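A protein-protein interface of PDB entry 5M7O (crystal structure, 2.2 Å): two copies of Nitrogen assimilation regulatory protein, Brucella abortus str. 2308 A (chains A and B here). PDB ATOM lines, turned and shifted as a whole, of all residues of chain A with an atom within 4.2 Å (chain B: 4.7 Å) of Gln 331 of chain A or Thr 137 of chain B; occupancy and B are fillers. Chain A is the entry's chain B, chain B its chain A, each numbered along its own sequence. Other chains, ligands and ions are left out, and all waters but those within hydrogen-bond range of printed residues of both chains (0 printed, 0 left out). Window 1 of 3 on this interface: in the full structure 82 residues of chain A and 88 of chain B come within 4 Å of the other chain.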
ATOM      1  N   ARG A 136     -21.995   6.521   2.802  1.00  0.00           N
ATOM      2  CA  ARG A 136     -21.864   7.744   2.007  1.00  0.00           C
ATOM      3  C   ARG A 136     -20.402   8.196   1.753  1.00  0.00           C
ATOM      4  O   ARG A 136     -19.696   7.698   0.860  1.00  0.00           O
ATOM      5  CB  ARG A 136     -22.629   8.856   2.728  1.00  0.00           C
ATOM      6  CG  ARG A 136     -24.127   8.554   2.965  1.00  0.00           C
ATOM      7  CD  ARG A 136     -24.831   9.571   3.851  1.00  0.00           C
ATOM      8  NE  ARG A 136     -24.197  10.888   3.764  1.00  0.00           N
ATOM      9  CZ  ARG A 136     -24.404  11.910   4.587  1.00  0.00           C
ATOM     10  NH1 ARG A 136     -25.268  11.809   5.600  1.00  0.00           N
ATOM     11  NH2 ARG A 136     -23.729  13.048   4.387  1.00  0.00           N
ATOM     12  N   GLN A 327     -25.964   5.598  -4.398  1.00  0.00           N
ATOM     13  CA  GLN A 327     -25.283   6.510  -3.470  1.00  0.00           C
ATOM     14  C   GLN A 327     -25.889   7.907  -3.435  1.00  0.00           C
ATOM     15  O   GLN A 327     -25.972   8.504  -2.368  1.00  0.00           O
ATOM     16  CB  GLN A 327     -23.780   6.569  -3.796  1.00  0.00           C
ATOM     17  CG  GLN A 327     -22.973   7.715  -3.179  1.00  0.00           C
ATOM     18  CD  GLN A 327     -21.451   7.535  -3.329  1.00  0.00           C
ATOM     19  OE1 GLN A 327     -20.770   8.318  -4.013  1.00  0.00           O
ATOM     20  NE2 GLN A 327     -20.917   6.499  -2.692  1.00  0.00           N
ATOM     21  N   ILE A 328     -26.296   8.424  -4.595  1.00  0.00           N
ATOM     22  CA  ILE A 328     -26.907   9.767  -4.692  1.00  0.00           C
ATOM     23  C   ILE A 328     -28.270   9.817  -3.966  1.00  0.00           C
ATOM     24  O   ILE A 328     -28.570  10.800  -3.285  1.00  0.00           O
ATOM     25  CB  ILE A 328     -27.076  10.247  -6.164  1.00  0.00           C
ATOM     26  CG1 ILE A 328     -25.718  10.425  -6.862  1.00  0.00           C
ATOM     27  CG2 ILE A 328     -27.850  11.561  -6.233  1.00  0.00           C
ATOM     28  CD1 ILE A 328     -24.929  11.670  -6.503  1.00  0.00           C
ATOM     29  N   ALA A 329     -29.082   8.774  -4.136  1.00  0.00           N
ATOM     30  CA  ALA A 329     -30.313   8.575  -3.351  1.00  0.00           C
ATOM     31  C   ALA A 329     -30.080   8.586  -1.836  1.00  0.00           C
ATOM     32  O   ALA A 329     -30.812   9.227  -1.097  1.00  0.00           O
ATOM     33  CB  ALA A 329     -30.946   7.268  -3.738  1.00  0.00           C
ATOM     34  N   GLU A 330     -29.067   7.860  -1.382  1.00  0.00           N
ATOM     35  CA  GLU A 330     -28.644   7.913   0.018  1.00  0.00           C
ATOM     36  C   GLU A 330     -28.359   9.360   0.425  1.00  0.00           C
ATOM     37  O   GLU A 330     -28.991   9.888   1.340  1.00  0.00           O
ATOM     38  CB  GLU A 330     -27.396   7.050   0.252  1.00  0.00           C
ATOM     39  N   GLN A 331     -27.437   9.999  -0.297  1.00  0.00           N
ATOM     40  CA  GLN A 331     -27.021  11.393  -0.028  1.00  0.00           C
ATOM     41  C   GLN A 331     -28.120  12.480  -0.189  1.00  0.00           C
ATOM     42  O   GLN A 331     -27.954  13.565   0.357  1.00  0.00           O
ATOM     43  CB  GLN A 331     -25.797  11.774  -0.896  1.00  0.00           C
ATOM     44  CG  GLN A 331     -24.449  11.196  -0.448  1.00  0.00           C
ATOM     45  CD  GLN A 331     -23.559  12.203   0.290  1.00  0.00           C
ATOM     46  OE1 GLN A 331     -23.401  12.139   1.510  1.00  0.00           O
ATOM     47  NE2 GLN A 331     -22.979  13.137  -0.452  1.00  0.00           N
ATOM     48  N   ALA A 332     -29.210  12.205  -0.923  1.00  0.00           N
ATOM     49  CA  ALA A 332     -30.212  13.247  -1.282  1.00  0.00           C
ATOM     50  C   ALA A 332     -31.706  12.881  -1.229  1.00  0.00           C
ATOM     51  O   ALA A 332     -32.560  13.726  -1.495  1.00  0.00           O
ATOM     52  CB  ALA A 332     -29.886  13.794  -2.670  1.00  0.00           C
ATOM     53  N   GLY A 333     -32.037  11.649  -0.889  1.00  0.00           N
ATOM     54  CA  GLY A 333     -33.447  11.236  -0.805  1.00  0.00           C
ATOM     55  C   GLY A 333     -34.219  11.135  -2.119  1.00  0.00           C
ATOM     56  O   GLY A 333     -35.448  11.153  -2.113  1.00  0.00           O
ATOM     57  N   ARG A 360     -20.065  10.916 -11.924  1.00  0.00           N
ATOM     58  CA  ARG A 360     -20.946  11.196 -10.768  1.00  0.00           C
ATOM     59  C   ARG A 360     -21.713  12.520 -10.920  1.00  0.00           C
ATOM     60  O   ARG A 360     -22.934  12.541 -10.754  1.00  0.00           O
ATOM     61  CB  ARG A 360     -20.157  11.223  -9.465  1.00  0.00           C
ATOM     62  CG  ARG A 360     -21.011  11.247  -8.205  1.00  0.00           C
ATOM     63  CD  ARG A 360     -20.146  11.304  -6.954  1.00  0.00           C
ATOM     64  NE  ARG A 360     -20.883  10.948  -5.728  1.00  0.00           N
ATOM     65  CZ  ARG A 360     -21.779  11.724  -5.096  1.00  0.00           C
ATOM     66  NH1 ARG A 360     -22.114  12.942  -5.560  1.00  0.00           N
ATOM     67  NH2 ARG A 360     -22.369  11.270  -3.984  1.00  0.00           N
ATOM     68  N   LEU B 133     -14.810  11.688   8.049  1.00  0.00           N
ATOM     69  CA  LEU B 133     -15.893  11.211   7.149  1.00  0.00           C
ATOM     70  C   LEU B 133     -16.959  12.253   6.864  1.00  0.00           C
ATOM     71  O   LEU B 133     -17.621  12.160   5.838  1.00  0.00           O
ATOM     72  CB  LEU B 133     -16.595   9.976   7.697  1.00  0.00           C
ATOM     73  CG  LEU B 133     -15.832   8.659   7.688  1.00  0.00           C
ATOM     74  CD1 LEU B 133     -16.763   7.543   8.123  1.00  0.00           C
ATOM     75  CD2 LEU B 133     -15.244   8.342   6.324  1.00  0.00           C
ATOM     76  N   ARG B 134     -17.123  13.209   7.780  1.00  0.00           N
ATOM     77  CA  ARG B 134     -18.008  14.350   7.606  1.00  0.00           C
ATOM     78  C   ARG B 134     -17.463  15.287   6.530  1.00  0.00           C
ATOM     79  O   ARG B 134     -18.201  15.690   5.629  1.00  0.00           O
ATOM     80  CB  ARG B 134     -18.147  15.095   8.934  1.00  0.00           C
ATOM     81  CG  ARG B 134     -19.285  16.107   9.010  1.00  0.00           C
ATOM     82  CD  ARG B 134     -19.716  16.344  10.459  1.00  0.00           C
ATOM     83  NE  ARG B 134     -20.438  15.187  11.010  1.00  0.00           N
ATOM     84  CZ  ARG B 134     -20.741  14.994  12.298  1.00  0.00           C
ATOM     85  NH1 ARG B 134     -20.385  15.875  13.232  1.00  0.00           N
ATOM     86  NH2 ARG B 134     -21.413  13.901  12.658  1.00  0.00           N
ATOM     87  N   LYS B 135     -16.180  15.640   6.638  1.00  0.00           N
ATOM     88  CA  LYS B 135     -15.498  16.482   5.636  1.00  0.00           C
ATOM     89  C   LYS B 135     -15.487  15.785   4.270  1.00  0.00           C
ATOM     90  O   LYS B 135     -15.700  16.436   3.243  1.00  0.00           O
ATOM     91  CB  LYS B 135     -14.070  16.869   6.081  1.00  0.00           C
ATOM     92  N   ARG B 136     -15.289  14.467   4.264  1.00  0.00           N
ATOM     93  CA  ARG B 136     -15.243  13.695   3.009  1.00  0.00           C
ATOM     94  C   ARG B 136     -16.588  13.377   2.363  1.00  0.00           C
ATOM     95  O   ARG B 136     -16.600  12.941   1.218  1.00  0.00           O
ATOM     96  CB  ARG B 136     -14.421  12.411   3.170  1.00  0.00           C
ATOM     97  CG  ARG B 136     -12.916  12.639   3.032  1.00  0.00           C
ATOM     98  CD  ARG B 136     -12.135  11.562   3.767  1.00  0.00           C
ATOM     99  NE  ARG B 136     -12.483  10.222   3.279  1.00  0.00           N
ATOM    100  CZ  ARG B 136     -12.492   9.104   4.004  1.00  0.00           C
ATOM    101  NH1 ARG B 136     -12.187   9.109   5.307  1.00  0.00           N
ATOM    102  NH2 ARG B 136     -12.825   7.958   3.410  1.00  0.00           N
ATOM    103  N   THR B 137     -17.705  13.565   3.068  1.00  0.00           N
ATOM    104  CA  THR B 137     -19.019  13.538   2.390  1.00  0.00           C
ATOM    105  C   THR B 137     -19.346  14.881   1.702  1.00  0.00           C
ATOM    106  O   THR B 137     -19.759  14.898   0.539  1.00  0.00           O
ATOM    107  CB  THR B 137     -20.214  13.117   3.295  1.00  0.00           C
ATOM    108  OG1 THR B 137     -20.309  13.949   4.468  1.00  0.00           O
ATOM    109  CG2 THR B 137     -20.098  11.636   3.645  1.00  0.00           C
ATOM    110  N   GLY B 138     -19.135  15.989   2.418  1.00  0.00           N
ATOM    111  CA  GLY B 138     -19.665  17.300   2.031  1.00  0.00           C
ATOM    112  C   GLY B 138     -21.184  17.353   2.225  1.00  0.00           C
ATOM    113  O   GLY B 138     -21.722  17.118   3.319  1.00  0.00           O
ATOM    114  N   GLN B 331     -13.982  17.910  -0.288  1.00  0.00           N
ATOM    115  CA  GLN B 331     -14.520  16.586  -0.645  1.00  0.00           C
ATOM    116  C   GLN B 331     -13.882  15.914  -1.865  1.00  0.00           C
ATOM    117  O   GLN B 331     -13.889  14.685  -1.950  1.00  0.00           O
ATOM    118  CB  GLN B 331     -16.033  16.666  -0.880  1.00  0.00           C
ATOM    119  CG  GLN B 331     -16.609  15.457  -1.616  1.00  0.00           C
ATOM    120  CD  GLN B 331     -18.088  15.551  -1.903  1.00  0.00           C
ATOM    121  OE1 GLN B 331     -18.638  16.642  -2.071  1.00  0.00           O
ATOM    122  NE2 GLN B 331     -18.747  14.391  -1.984  1.00  0.00           N
ATOM    123  N   ARG B 357     -29.591  21.784  -3.862  1.00  0.00           N
ATOM    124  CA  ARG B 357     -28.962  20.621  -4.550  1.00  0.00           C
ATOM    125  C   ARG B 357     -28.538  20.975  -5.969  1.00  0.00           C
ATOM    126  O   ARG B 357     -27.442  20.612  -6.414  1.00  0.00           O
ATOM    127  CB  ARG B 357     -29.885  19.411  -4.686  1.00  0.00           C
ATOM    128  CG  ARG B 357     -30.556  18.942  -3.416  1.00  0.00           C
ATOM    129  CD  ARG B 357     -29.869  17.752  -2.777  1.00  0.00           C
ATOM    130  NE  ARG B 357     -29.964  17.833  -1.312  1.00  0.00           N
ATOM    131  CZ  ARG B 357     -29.283  17.067  -0.460  1.00  0.00           C
ATOM    132  NH1 ARG B 357     -28.452  16.124  -0.905  1.00  0.00           N
ATOM    133  NH2 ARG B 357     -29.445  17.236   0.847  1.00  0.00           N
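The guanidinium group of Arg 357 of chain B lies within hydrogen-bond range of the backbone carbonyl oxygen of Gln 331 of chain A (2.9 Å).
The side-chain hydroxyl of Thr 137 of chain B sits at hydrogen-bond distance from the backbone carbonyl oxygen of Arg 134 of chain B (3.0 Å). The backbone carbonyl oxygen of Thr 137 of chain B sits at hydrogen-bond distance from the side-chain amide nitrogen of Gln 331 of chain B (2.8 Å). The side-chain amide oxygen of Gln 331 of chain A sits at hydrogen-bond distance from the guanidinium group of Arg 136 of chain A (2.7 Å).
Arg 136 of chain A touches Thr 137 of chain B. OE1 of Gln 331 of chain A touches CB of Thr 137 of chain B, at 3.8 Å. Arg 357 of chain B touches Ala 332 of chain A.
Printed residues of chain B within 4 Å of Arg 136 of chain A: Thr 137 (3.5 Å). Glu 330 of chain A touches none of the printed residues of chain B. Of chain B, only Thr 137 and Arg 357 come within 4 Å of Gln 331 of chain A. Of the printed residues of chain B, Ala 332 of chain A touches Arg 357 (3.3 Å). Of the printed residues of chain A, Thr 137 of chain B touches Arg 136 and Gln 331. Of the printed residues of chain A, Arg 357 of chain B touches Gln 331 and Ala 332. The nearest printed residue of chain B that does not touch Gln 331 of chain A is Gln 331 of chain B (4.7 Å). The nearest printed residue of chain B that does not touch Ala 332 of chain A is Gly 138 of chain B (9.9 Å).
Printed residues of chain B that touch a printed residue of chain A: Thr 137 and Arg 357. Along chain B the printed residues that touch a printed residue of chain A span positions 137 to 357. Printed residues of chain A that touch a printed residue of chain B: Arg 136, Gln 331 and Ala 332. Hydrophobic or aromatic side chains of chain A that line the printed part of chain B: Ala 332. Among the printed residues, no Asp or Glu carboxylate lies within 4 Å of a Lys or Arg side-chain nitrogen of the other chain.
2 positions are printed for both chains. Of the 4 pairs that touch across the chains among the printed residues, none has its exchanged pair printed and touching as well.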
